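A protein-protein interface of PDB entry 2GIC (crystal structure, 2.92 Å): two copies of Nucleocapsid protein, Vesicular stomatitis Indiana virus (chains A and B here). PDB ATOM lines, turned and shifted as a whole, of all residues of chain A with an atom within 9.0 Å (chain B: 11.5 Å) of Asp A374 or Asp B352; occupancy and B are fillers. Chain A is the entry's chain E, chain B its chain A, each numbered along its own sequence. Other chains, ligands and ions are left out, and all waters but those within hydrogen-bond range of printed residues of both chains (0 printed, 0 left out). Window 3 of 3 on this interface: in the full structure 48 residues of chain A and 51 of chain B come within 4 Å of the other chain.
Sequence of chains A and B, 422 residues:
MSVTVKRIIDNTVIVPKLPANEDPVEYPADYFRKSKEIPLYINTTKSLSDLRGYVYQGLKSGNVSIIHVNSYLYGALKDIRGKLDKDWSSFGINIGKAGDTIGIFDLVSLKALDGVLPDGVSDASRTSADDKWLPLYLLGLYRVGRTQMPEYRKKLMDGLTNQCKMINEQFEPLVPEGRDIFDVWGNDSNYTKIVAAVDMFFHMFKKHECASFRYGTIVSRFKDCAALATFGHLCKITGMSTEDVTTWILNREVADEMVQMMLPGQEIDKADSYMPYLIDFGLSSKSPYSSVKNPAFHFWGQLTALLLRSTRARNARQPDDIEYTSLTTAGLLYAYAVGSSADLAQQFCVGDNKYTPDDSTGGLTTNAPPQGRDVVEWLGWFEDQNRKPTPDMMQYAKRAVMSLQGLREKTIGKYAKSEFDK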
ATOM      1  N   MET A 240     -10.482  16.434   3.813  1.00  0.00           N
ATOM      2  CA  MET A 240      -9.258  16.538   4.586  1.00  0.00           C
ATOM      3  C   MET A 240      -9.236  15.494   5.685  1.00  0.00           C
ATOM      4  O   MET A 240     -10.284  15.000   6.113  1.00  0.00           O
ATOM      5  CB  MET A 240      -9.130  17.932   5.197  1.00  0.00           C
ATOM      6  CG  MET A 240      -9.115  19.067   4.180  1.00  0.00           C
ATOM      7  SD  MET A 240      -8.663  20.635   4.935  1.00  0.00           S
ATOM      8  CE  MET A 240      -6.872  20.578   4.834  1.00  0.00           C
ATOM      9  N   GLU A 243      -6.581  15.111  11.172  1.00  0.00           N
ATOM     10  CA  GLU A 243      -5.496  15.948  11.689  1.00  0.00           C
ATOM     11  C   GLU A 243      -5.364  17.273  10.937  1.00  0.00           C
ATOM     12  O   GLU A 243      -5.003  18.293  11.534  1.00  0.00           O
ATOM     13  CB  GLU A 243      -4.159  15.195  11.733  1.00  0.00           C
ATOM     14  CG  GLU A 243      -3.968  14.129  10.668  1.00  0.00           C
ATOM     15  CD  GLU A 243      -4.551  12.781  11.065  1.00  0.00           C
ATOM     16  OE1 GLU A 243      -4.970  12.631  12.237  1.00  0.00           O
ATOM     17  OE2 GLU A 243      -4.587  11.872  10.201  1.00  0.00           O
ATOM     18  N   ASP A 244      -5.658  17.249   9.637  1.00  0.00           N
ATOM     19  CA  ASP A 244      -5.702  18.470   8.826  1.00  0.00           C
ATOM     20  C   ASP A 244      -6.822  19.399   9.274  1.00  0.00           C
ATOM     21  O   ASP A 244      -6.621  20.608   9.398  1.00  0.00           O
ATOM     22  CB  ASP A 244      -5.862  18.144   7.338  1.00  0.00           C
ATOM     23  CG  ASP A 244      -4.534  18.067   6.613  1.00  0.00           C
ATOM     24  OD1 ASP A 244      -3.875  19.122   6.472  1.00  0.00           O
ATOM     25  OD2 ASP A 244      -4.154  16.957   6.174  1.00  0.00           O
ATOM     26  N   THR A 247      -6.015  21.207  12.596  1.00  0.00           N
ATOM     27  CA  THR A 247      -5.120  22.349  12.427  1.00  0.00           C
ATOM     28  C   THR A 247      -5.839  23.565  11.838  1.00  0.00           C
ATOM     29  O   THR A 247      -5.340  24.686  11.925  1.00  0.00           O
ATOM     30  CB  THR A 247      -3.913  22.004  11.542  1.00  0.00           C
ATOM     31  OG1 THR A 247      -4.364  21.681  10.219  1.00  0.00           O
ATOM     32  CG2 THR A 247      -3.119  20.831  12.136  1.00  0.00           C
ATOM     33  N   TRP A 248      -7.011  23.348  11.249  1.00  0.00           N
ATOM     34  CA  TRP A 248      -7.798  24.447  10.710  1.00  0.00           C
ATOM     35  C   TRP A 248      -8.738  25.114  11.725  1.00  0.00           C
ATOM     36  O   TRP A 248      -9.466  26.069  11.393  1.00  0.00           O
ATOM     37  CB  TRP A 248      -8.546  24.005   9.457  1.00  0.00           C
ATOM     38  CG  TRP A 248      -7.819  24.412   8.218  1.00  0.00           C
ATOM     39  CD1 TRP A 248      -6.986  23.638   7.453  1.00  0.00           C
ATOM     40  CD2 TRP A 248      -7.842  25.705   7.606  1.00  0.00           C
ATOM     41  NE1 TRP A 248      -6.496  24.373   6.399  1.00  0.00           N
ATOM     42  CE2 TRP A 248      -7.004  25.644   6.467  1.00  0.00           C
ATOM     43  CE3 TRP A 248      -8.499  26.911   7.904  1.00  0.00           C
ATOM     44  CZ2 TRP A 248      -6.803  26.743   5.627  1.00  0.00           C
ATOM     45  CZ3 TRP A 248      -8.298  28.002   7.072  1.00  0.00           C
ATOM     46  CH2 TRP A 248      -7.456  27.909   5.943  1.00  0.00           C
ATOM     47  N   LEU A 250      -9.373  27.694  14.290  1.00  0.00           N
ATOM     48  CA  LEU A 250      -8.710  28.991  14.429  1.00  0.00           C
ATOM     49  C   LEU A 250      -9.180  29.808  15.629  1.00  0.00           C
ATOM     50  O   LEU A 250      -8.643  30.886  15.900  1.00  0.00           O
ATOM     51  CB  LEU A 250      -8.815  29.794  13.129  1.00  0.00           C
ATOM     52  CG  LEU A 250      -8.047  29.189  11.947  1.00  0.00           C
ATOM     53  CD1 LEU A 250      -8.536  29.741  10.609  1.00  0.00           C
ATOM     54  CD2 LEU A 250      -6.530  29.374  12.095  1.00  0.00           C
ATOM     55  N   LEU A 333     -12.940  31.691   5.772  1.00  0.00           N
ATOM     56  CA  LEU A 333     -11.549  31.452   5.366  1.00  0.00           C
ATOM     57  C   LEU A 333     -11.256  29.971   5.091  1.00  0.00           C
ATOM     58  O   LEU A 333     -10.623  29.645   4.080  1.00  0.00           O
ATOM     59  CB  LEU A 333     -10.572  32.010   6.404  1.00  0.00           C
ATOM     60  CG  LEU A 333      -9.084  31.896   6.042  1.00  0.00           C
ATOM     61  CD1 LEU A 333      -8.668  33.024   5.097  1.00  0.00           C
ATOM     62  CD2 LEU A 333      -8.208  31.879   7.297  1.00  0.00           C
ATOM     63  N   TYR A 334     -11.727  29.092   5.979  1.00  0.00           N
ATOM     64  CA  TYR A 334     -11.647  27.653   5.758  1.00  0.00           C
ATOM     65  C   TYR A 334     -12.382  27.231   4.480  1.00  0.00           C
ATOM     66  O   TYR A 334     -11.801  26.578   3.607  1.00  0.00           O
ATOM     67  CB  TYR A 334     -12.173  26.880   6.979  1.00  0.00           C
ATOM     68  CG  TYR A 334     -11.798  25.405   7.004  1.00  0.00           C
ATOM     69  CD1 TYR A 334     -10.766  24.907   6.200  1.00  0.00           C
ATOM     70  CD2 TYR A 334     -12.456  24.521   7.845  1.00  0.00           C
ATOM     71  CE1 TYR A 334     -10.418  23.569   6.216  1.00  0.00           C
ATOM     72  CE2 TYR A 334     -12.112  23.172   7.874  1.00  0.00           C
ATOM     73  CZ  TYR A 334     -11.088  22.699   7.059  1.00  0.00           C
ATOM     74  OH  TYR A 334     -10.730  21.359   7.083  1.00  0.00           O
ATOM     75  N   ALA A 337     -10.710  28.452   1.298  1.00  0.00           N
ATOM     76  CA  ALA A 337      -9.453  27.749   1.005  1.00  0.00           C
ATOM     77  C   ALA A 337      -9.703  26.405   0.323  1.00  0.00           C
ATOM     78  O   ALA A 337      -9.232  26.164  -0.792  1.00  0.00           O
ATOM     79  CB  ALA A 337      -8.624  27.563   2.273  1.00  0.00           C
ATOM     80  N   VAL A 338     -10.456  25.544   0.998  1.00  0.00           N
ATOM     81  CA  VAL A 338     -10.865  24.265   0.442  1.00  0.00           C
ATOM     82  C   VAL A 338     -11.527  24.481  -0.923  1.00  0.00           C
ATOM     83  O   VAL A 338     -11.189  23.803  -1.902  1.00  0.00           O
ATOM     84  CB  VAL A 338     -11.821  23.523   1.427  1.00  0.00           C
ATOM     85  CG1 VAL A 338     -12.536  22.360   0.758  1.00  0.00           C
ATOM     86  CG2 VAL A 338     -11.053  23.042   2.656  1.00  0.00           C
ATOM     87  N   SER A 341      -9.010  25.787  -3.615  1.00  0.00           N
ATOM     88  CA  SER A 341      -7.969  24.795  -3.853  1.00  0.00           C
ATOM     89  C   SER A 341      -8.597  23.433  -4.099  1.00  0.00           C
ATOM     90  O   SER A 341      -8.725  22.619  -3.184  1.00  0.00           O
ATOM     91  CB  SER A 341      -6.984  24.731  -2.687  1.00  0.00           C
ATOM     92  OG  SER A 341      -6.260  25.937  -2.577  1.00  0.00           O
ATOM     93  N   PRO A 370      -3.055  31.508  -2.253  1.00  0.00           N
ATOM     94  CA  PRO A 370      -2.099  30.484  -1.811  1.00  0.00           C
ATOM     95  C   PRO A 370      -2.305  29.127  -2.488  1.00  0.00           C
ATOM     96  O   PRO A 370      -3.444  28.733  -2.771  1.00  0.00           O
ATOM     97  CB  PRO A 370      -2.363  30.363  -0.309  1.00  0.00           C
ATOM     98  CG  PRO A 370      -3.062  31.605   0.064  1.00  0.00           C
ATOM     99  CD  PRO A 370      -3.841  32.045  -1.132  1.00  0.00           C
ATOM    100  N   GLN A 371      -1.183  28.442  -2.714  1.00  0.00           N
ATOM    101  CA  GLN A 371      -1.076  27.158  -3.422  1.00  0.00           C
ATOM    102  C   GLN A 371      -2.197  26.160  -3.129  1.00  0.00           C
ATOM    103  O   GLN A 371      -3.136  26.025  -3.912  1.00  0.00           O
ATOM    104  CB  GLN A 371       0.268  26.498  -3.083  1.00  0.00           C
ATOM    105  CG  GLN A 371       1.363  27.463  -2.601  1.00  0.00           C
ATOM    106  CD  GLN A 371       2.543  26.743  -1.963  1.00  0.00           C
ATOM    107  OE1 GLN A 371       2.371  25.862  -1.115  1.00  0.00           O
ATOM    108  NE2 GLN A 371       3.751  27.124  -2.364  1.00  0.00           N
ATOM    109  N   GLY A 372      -2.081  25.462  -2.002  1.00  0.00           N
ATOM    110  CA  GLY A 372      -2.985  24.375  -1.660  1.00  0.00           C
ATOM    111  C   GLY A 372      -3.804  24.701  -0.434  1.00  0.00           C
ATOM    112  O   GLY A 372      -4.475  25.735  -0.394  1.00  0.00           O
ATOM    113  N   ARG A 373      -3.739  23.828   0.572  1.00  0.00           N
ATOM    114  CA  ARG A 373      -4.615  23.936   1.740  1.00  0.00           C
ATOM    115  C   ARG A 373      -3.919  23.847   3.114  1.00  0.00           C
ATOM    116  O   ARG A 373      -4.502  23.328   4.070  1.00  0.00           O
ATOM    117  CB  ARG A 373      -5.721  22.876   1.665  1.00  0.00           C
ATOM    118  CG  ARG A 373      -6.647  22.942   0.461  1.00  0.00           C
ATOM    119  CD  ARG A 373      -7.807  21.997   0.695  1.00  0.00           C
ATOM    120  NE  ARG A 373      -8.396  21.462  -0.528  1.00  0.00           N
ATOM    121  CZ  ARG A 373      -9.413  20.604  -0.546  1.00  0.00           C
ATOM    122  NH1 ARG A 373      -9.955  20.181   0.588  1.00  0.00           N
ATOM    123  NH2 ARG A 373      -9.898  20.162  -1.695  1.00  0.00           N
ATOM    124  N   ASP A 374      -2.694  24.347   3.232  1.00  0.00           N
ATOM    125  CA  ASP A 374      -2.063  24.398   4.548  1.00  0.00           C
ATOM    126  C   ASP A 374      -2.467  25.661   5.325  1.00  0.00           C
ATOM    127  O   ASP A 374      -2.475  26.764   4.769  1.00  0.00           O
ATOM    128  CB  ASP A 374      -0.543  24.296   4.439  1.00  0.00           C
ATOM    129  CG  ASP A 374       0.139  24.233   5.801  1.00  0.00           C
ATOM    130  OD1 ASP A 374       1.282  24.718   5.914  1.00  0.00           O
ATOM    131  OD2 ASP A 374      -0.465  23.710   6.764  1.00  0.00           O
ATOM    132  N   VAL A 375      -2.785  25.491   6.610  1.00  0.00           N
ATOM    133  CA  VAL A 375      -3.284  26.594   7.456  1.00  0.00           C
ATOM    134  C   VAL A 375      -2.267  27.723   7.590  1.00  0.00           C
ATOM    135  O   VAL A 375      -2.631  28.905   7.629  1.00  0.00           O
ATOM    136  CB  VAL A 375      -3.659  26.134   8.898  1.00  0.00           C
ATOM    137  CG1 VAL A 375      -4.815  26.958   9.435  1.00  0.00           C
ATOM    138  CG2 VAL A 375      -4.005  24.661   8.930  1.00  0.00           C
ATOM    139  N   VAL A 376      -0.998  27.337   7.666  1.00  0.00           N
ATOM    140  CA  VAL A 376       0.088  28.270   7.900  1.00  0.00           C
ATOM    141  C   VAL A 376       0.206  29.274   6.758  1.00  0.00           C
ATOM    142  O   VAL A 376       0.312  30.478   6.999  1.00  0.00           O
ATOM    143  CB  VAL A 376       1.407  27.517   8.133  1.00  0.00           C
ATOM    144  CG1 VAL A 376       2.576  28.482   8.236  1.00  0.00           C
ATOM    145  CG2 VAL A 376       1.302  26.673   9.394  1.00  0.00           C
ATOM    146  N   GLU A 377       0.161  28.776   5.523  1.00  0.00           N
ATOM    147  CA  GLU A 377       0.230  29.628   4.332  1.00  0.00           C
ATOM    148  C   GLU A 377      -0.967  30.582   4.210  1.00  0.00           C
ATOM    149  O   GLU A 377      -0.802  31.769   3.905  1.00  0.00           O
ATOM    150  CB  GLU A 377       0.363  28.781   3.064  1.00  0.00           C
ATOM    151  CG  GLU A 377       1.789  28.384   2.725  1.00  0.00           C
ATOM    152  CD  GLU A 377       1.956  27.981   1.268  1.00  0.00           C
ATOM    153  OE1 GLU A 377       1.018  27.379   0.701  1.00  0.00           O
ATOM    154  OE2 GLU A 377       3.028  28.266   0.688  1.00  0.00           O
ATOM    155  N   TRP A 378      -2.164  30.065   4.454  1.00  0.00           N
ATOM    156  CA  TRP A 378      -3.362  30.880   4.379  1.00  0.00           C
ATOM    157  C   TRP A 378      -3.436  31.921   5.496  1.00  0.00           C
ATOM    158  O   TRP A 378      -3.926  33.036   5.284  1.00  0.00           O
ATOM    159  CB  TRP A 378      -4.594  29.987   4.387  1.00  0.00           C
ATOM    160  CG  TRP A 378      -4.852  29.392   3.062  1.00  0.00           C
ATOM    161  CD1 TRP A 378      -4.391  28.196   2.593  1.00  0.00           C
ATOM    162  CD2 TRP A 378      -5.617  29.974   2.007  1.00  0.00           C
ATOM    163  NE1 TRP A 378      -4.833  27.988   1.309  1.00  0.00           N
ATOM    164  CE2 TRP A 378      -5.587  29.067   0.923  1.00  0.00           C
ATOM    165  CE3 TRP A 378      -6.329  31.172   1.871  1.00  0.00           C
ATOM    166  CZ2 TRP A 378      -6.246  29.322  -0.285  1.00  0.00           C
ATOM    167  CZ3 TRP A 378      -6.987  31.425   0.670  1.00  0.00           C
ATOM    168  CH2 TRP A 378      -6.941  30.502  -0.389  1.00  0.00           C
ATOM    169  N   LEU A 379      -2.948  31.553   6.680  1.00  0.00           N
ATOM    170  CA  LEU A 379      -2.935  32.466   7.822  1.00  0.00           C
ATOM    171  C   LEU A 379      -2.010  33.642   7.561  1.00  0.00           C
ATOM    172  O   LEU A 379      -2.241  34.743   8.067  1.00  0.00           O
ATOM    173  CB  LEU A 379      -2.498  31.749   9.098  1.00  0.00           C
ATOM    174  CG  LEU A 379      -3.529  31.053   9.981  1.00  0.00           C
ATOM    175  CD1 LEU A 379      -2.788  30.350  11.097  1.00  0.00           C
ATOM    176  CD2 LEU A 379      -4.548  32.040  10.551  1.00  0.00           C
ATOM    177  N   GLY A 380      -0.961  33.395   6.781  1.00  0.00           N
ATOM    178  CA  GLY A 380      -0.037  34.442   6.380  1.00  0.00           C
ATOM    179  C   GLY A 380      -0.667  35.308   5.314  1.00  0.00           C
ATOM    180  O   GLY A 380      -0.573  36.533   5.365  1.00  0.00           O
ATOM    181  N   TRP A 381      -1.318  34.660   4.351  1.00  0.00           N
ATOM    182  CA  TRP A 381      -2.029  35.351   3.277  1.00  0.00           C
ATOM    183  C   TRP A 381      -3.176  36.211   3.798  1.00  0.00           C
ATOM    184  O   TRP A 381      -3.449  37.279   3.252  1.00  0.00           O
ATOM    185  CB  TRP A 381      -2.565  34.345   2.265  1.00  0.00           C
ATOM    186  CG  TRP A 381      -3.372  34.969   1.166  1.00  0.00           C
ATOM    187  CD1 TRP A 381      -2.893  35.515   0.014  1.00  0.00           C
ATOM    188  CD2 TRP A 381      -4.800  35.107   1.113  1.00  0.00           C
ATOM    189  NE1 TRP A 381      -3.930  35.986  -0.757  1.00  0.00           N
ATOM    190  CE2 TRP A 381      -5.112  35.748  -0.106  1.00  0.00           C
ATOM    191  CE3 TRP A 381      -5.846  34.753   1.977  1.00  0.00           C
ATOM    192  CZ2 TRP A 381      -6.427  36.040  -0.485  1.00  0.00           C
ATOM    193  CZ3 TRP A 381      -7.155  35.048   1.600  1.00  0.00           C
ATOM    194  CH2 TRP A 381      -7.431  35.683   0.380  1.00  0.00           C
ATOM    195  N   LEU B 344      -8.845  34.657  15.670  1.00  0.00           N
ATOM    196  CA  LEU B 344      -8.017  33.995  14.662  1.00  0.00           C
ATOM    197  C   LEU B 344      -6.548  33.792  15.035  1.00  0.00           C
ATOM    198  O   LEU B 344      -5.712  34.682  14.871  1.00  0.00           O
ATOM    199  CB  LEU B 344      -8.154  34.716  13.316  1.00  0.00           C
ATOM    200  CG  LEU B 344      -9.302  34.304  12.386  1.00  0.00           C
ATOM    201  CD1 LEU B 344      -8.823  33.250  11.405  1.00  0.00           C
ATOM    202  CD2 LEU B 344     -10.567  33.828  13.128  1.00  0.00           C
ATOM    203  N   ALA B 345      -6.257  32.603  15.551  1.00  0.00           N
ATOM    204  CA  ALA B 345      -4.896  32.162  15.838  1.00  0.00           C
ATOM    205  C   ALA B 345      -4.827  30.661  15.575  1.00  0.00           C
ATOM    206  O   ALA B 345      -5.812  29.940  15.784  1.00  0.00           O
ATOM    207  CB  ALA B 345      -4.530  32.468  17.271  1.00  0.00           C
ATOM    208  N   GLN B 346      -3.678  30.190  15.099  1.00  0.00           N
ATOM    209  CA  GLN B 346      -3.510  28.761  14.896  1.00  0.00           C
ATOM    210  C   GLN B 346      -3.514  28.084  16.262  1.00  0.00           C
ATOM    211  O   GLN B 346      -2.803  28.518  17.178  1.00  0.00           O
ATOM    212  CB  GLN B 346      -2.233  28.438  14.126  1.00  0.00           C
ATOM    213  CG  GLN B 346      -2.273  27.051  13.507  1.00  0.00           C
ATOM    214  CD  GLN B 346      -0.974  26.630  12.860  1.00  0.00           C
ATOM    215  OE1 GLN B 346      -0.079  27.442  12.640  1.00  0.00           O
ATOM    216  NE2 GLN B 346      -0.868  25.349  12.541  1.00  0.00           N
ATOM    217  N   GLN B 347      -4.322  27.035  16.395  1.00  0.00           N
ATOM    218  CA  GLN B 347      -4.504  26.362  17.679  1.00  0.00           C
ATOM    219  C   GLN B 347      -3.748  25.027  17.788  1.00  0.00           C
ATOM    220  O   GLN B 347      -3.269  24.666  18.869  1.00  0.00           O
ATOM    221  CB  GLN B 347      -5.996  26.172  17.964  1.00  0.00           C
ATOM    222  CG  GLN B 347      -6.823  27.456  17.906  1.00  0.00           C
ATOM    223  CD  GLN B 347      -6.531  28.409  19.055  1.00  0.00           C
ATOM    224  OE1 GLN B 347      -6.195  29.576  18.841  1.00  0.00           O
ATOM    225  NE2 GLN B 347      -6.652  27.912  20.282  1.00  0.00           N
ATOM    226  N   PHE B 348      -3.653  24.310  16.667  1.00  0.00           N
ATOM    227  CA  PHE B 348      -2.937  23.030  16.583  1.00  0.00           C
ATOM    228  C   PHE B 348      -1.940  23.038  15.417  1.00  0.00           C
ATOM    229  O   PHE B 348      -1.963  23.942  14.584  1.00  0.00           O
ATOM    230  CB  PHE B 348      -3.925  21.867  16.423  1.00  0.00           C
ATOM    231  CG  PHE B 348      -5.042  21.865  17.434  1.00  0.00           C
ATOM    232  CD1 PHE B 348      -6.225  22.555  17.186  1.00  0.00           C
ATOM    233  CD2 PHE B 348      -4.914  21.168  18.629  1.00  0.00           C
ATOM    234  CE1 PHE B 348      -7.262  22.556  18.112  1.00  0.00           C
ATOM    235  CE2 PHE B 348      -5.946  21.162  19.563  1.00  0.00           C
ATOM    236  CZ  PHE B 348      -7.123  21.859  19.303  1.00  0.00           C
ATOM    237  N   CYS B 349      -1.076  22.025  15.357  1.00  0.00           N
ATOM    238  CA  CYS B 349      -0.034  21.936  14.324  1.00  0.00           C
ATOM    239  C   CYS B 349       0.565  20.536  14.225  1.00  0.00           C
ATOM    240  O   CYS B 349       0.211  19.646  14.999  1.00  0.00           O
ATOM    241  CB  CYS B 349       1.087  22.924  14.636  1.00  0.00           C
ATOM    242  SG  CYS B 349       1.894  22.576  16.209  1.00  0.00           S
ATOM    243  N   VAL B 350       1.473  20.352  13.268  1.00  0.00           N
ATOM    244  CA  VAL B 350       2.286  19.132  13.178  1.00  0.00           C
ATOM    245  C   VAL B 350       3.782  19.502  13.137  1.00  0.00           C
ATOM    246  O   VAL B 350       4.521  19.097  12.238  1.00  0.00           O
ATOM    247  CB  VAL B 350       1.888  18.243  11.964  1.00  0.00           C
ATOM    248  CG1 VAL B 350       2.425  16.823  12.141  1.00  0.00           C
ATOM    249  CG2 VAL B 350       0.374  18.202  11.783  1.00  0.00           C
ATOM    250  N   GLY B 351       4.213  20.278  14.129  1.00  0.00           N
ATOM    251  CA  GLY B 351       5.563  20.837  14.158  1.00  0.00           C
ATOM    252  C   GLY B 351       5.715  22.076  13.286  1.00  0.00           C
ATOM    253  O   GLY B 351       6.799  22.650  13.205  1.00  0.00           O
ATOM    254  N   ASP B 352       4.622  22.488  12.644  1.00  0.00           N
ATOM    255  CA  ASP B 352       4.612  23.613  11.706  1.00  0.00           C
ATOM    256  C   ASP B 352       3.600  24.669  12.153  1.00  0.00           C
ATOM    257  O   ASP B 352       2.393  24.530  11.918  1.00  0.00           O
ATOM    258  CB  ASP B 352       4.290  23.104  10.294  1.00  0.00           C
ATOM    259  CG  ASP B 352       3.994  24.225   9.301  1.00  0.00           C
ATOM    260  OD1 ASP B 352       4.662  25.279   9.350  1.00  0.00           O
ATOM    261  OD2 ASP B 352       3.092  24.042   8.457  1.00  0.00           O
ATOM    262  N   ASN B 353       4.099  25.719  12.806  1.00  0.00           N
ATOM    263  CA  ASN B 353       3.239  26.755  13.390  1.00  0.00           C
ATOM    264  C   ASN B 353       3.416  28.099  12.692  1.00  0.00           C
ATOM    265  O   ASN B 353       4.525  28.442  12.275  1.00  0.00           O
ATOM    266  CB  ASN B 353       3.506  26.951  14.898  1.00  0.00           C
ATOM    267  CG  ASN B 353       4.265  25.783  15.551  1.00  0.00           C
ATOM    268  OD1 ASN B 353       4.160  24.627  15.136  1.00  0.00           O
ATOM    269  ND2 ASN B 353       5.028  26.098  16.596  1.00  0.00           N
ATOM    270  N   LYS B 354       2.331  28.865  12.576  1.00  0.00           N
ATOM    271  CA  LYS B 354       2.439  30.239  12.091  1.00  0.00           C
ATOM    272  C   LYS B 354       2.888  31.161  13.221  1.00  0.00           C
ATOM    273  O   LYS B 354       2.083  31.527  14.082  1.00  0.00           O
ATOM    274  CB  LYS B 354       1.124  30.750  11.491  1.00  0.00           C
ATOM    275  CG  LYS B 354       1.264  32.144  10.870  1.00  0.00           C
ATOM    276  CD  LYS B 354       0.037  33.017  11.122  1.00  0.00           C
ATOM    277  CE  LYS B 354       0.379  34.511  11.152  1.00  0.00           C
ATOM    278  NZ  LYS B 354       1.066  34.999   9.926  1.00  0.00           N
ATOM    279  N   TYR B 355       4.173  31.512  13.227  1.00  0.00           N
ATOM    280  CA  TYR B 355       4.674  32.547  14.122  1.00  0.00           C
ATOM    281  C   TYR B 355       4.238  33.875  13.518  1.00  0.00           C
ATOM    282  O   TYR B 355       4.557  34.174  12.364  1.00  0.00           O
ATOM    283  CB  TYR B 355       6.198  32.466  14.258  1.00  0.00           C
ATOM    284  CG  TYR B 355       6.736  32.989  15.580  1.00  0.00           C
ATOM    285  CD1 TYR B 355       6.593  32.247  16.758  1.00  0.00           C
ATOM    286  CD2 TYR B 355       7.403  34.218  15.651  1.00  0.00           C
ATOM    287  CE1 TYR B 355       7.089  32.721  17.978  1.00  0.00           C
ATOM    288  CE2 TYR B 355       7.903  34.702  16.867  1.00  0.00           C
ATOM    289  CZ  TYR B 355       7.742  33.947  18.025  1.00  0.00           C
ATOM    290  OH  TYR B 355       8.230  34.410  19.228  1.00  0.00           O
ATOM    291  N   THR B 356       3.496  34.659  14.291  1.00  0.00           N
ATOM    292  CA  THR B 356       2.755  35.799  13.738  1.00  0.00           C
ATOM    293  C   THR B 356       3.541  37.085  13.389  1.00  0.00           C
ATOM    294  O   THR B 356       3.313  37.648  12.315  1.00  0.00           O
ATOM    295  CB  THR B 356       1.454  36.115  14.546  1.00  0.00           C
ATOM    296  OG1 THR B 356       0.866  37.331  14.067  1.00  0.00           O
ATOM    297  CG2 THR B 356       1.731  36.243  16.038  1.00  0.00           C
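N of Ala B345 sits at hydrogen-bond distance from O of Leu A250, 3.0 Å away.
The side-chain carboxylate of Asp A374 sits close to the side-chain carboxylate of Asp B352, at 3.2 Å.
The backbone NH (N) of Lys B354 lies within hydrogen-bond range of the side-chain amide oxygen (OE1) of Gln B346, at 2.8 Å.
O of Asp A244 sits at hydrogen-bond distance from OG1 of Thr A247, at 2.6 Å.
The backbone carbonyl oxygen of Phe B348 sits at hydrogen-bond distance from the side-chain amide nitrogen of Gln B346 (2.7 Å).
NE2 of Gln B346 is in hydrogen-bond range of O of Asp B352, 3.4 Å away.
The backbone carbonyl oxygen (O) of Ala B345 sits close to the side-chain amide oxygen (OE1) of Gln B347.
SG of Cys B349 lies within hydrogen-bond range of OD1 of Asn B353 (3.2 Å).
Asp A374 touches just one residue of chain B: Asp B352 (3.2 Å).
Asp B352 touches just these residues of chain A: Asp A374 and Val A376.
Val A375 touches none of the printed residues of chain B.
No residue of chain A comes within 4 Å of Gly B351.
No residue of chain A comes within 4 Å of Asn B353.
Printed residues of chain A within 4 Å of Gln B346: Val A376 and Leu A379.
Of the printed residues of chain B, Leu A250 touches Leu B344 and Ala B345.
Of the printed residues of chain B, Val A376 touches Gln B346, Asp B352 and Lys B354.
Printed residues of chain A within 4 Å of Cys B349: Thr A247.
Arg A373 touches none of the printed residues of chain B.
The nearest residue of chain B that does not touch Asp A374 is Gln B346 (6.0 Å).
The nearest printed residue of chain A that does not touch Leu B344 is Leu A333 (4.4 Å).
No position is printed for both chains.
Of the 10 pairs that touch across the chains among the printed residues, none has its exchanged pair printed and touching as well.
Among the printed residues, pairs that only touch across the chains: Val A376 with Asp B352, Leu A250 with Leu B344, Leu A379 with Lys B354, Val A376 with Gln B346, Leu A379 with Gln B346, Gly A380 with Lys B354, Thr A247 with Cys B349 and Val A376 with Lys B354.
Of the 23 printed residues of chain A, 6 touch a printed residue of chain B.
Printed residues of chain A that touch a printed residue of chain B: Thr A247, Leu A250, Asp A374, Val A376, Leu A379 and Gly A380.
Hydrophobic or aromatic side chains of chain A that line the printed part of chain B: Leu A250, Val A376 and Leu A379.
Along chain A the printed residues that touch a printed residue of chain B span positions 247 to 380.
Of the 13 printed residues of chain B, 6 touch a printed residue of chain A.
Printed residues of chain B that touch a printed residue of chain A: Leu B344, Ala B345, Gln B346, Cys B349, Asp B352 and Lys B354.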
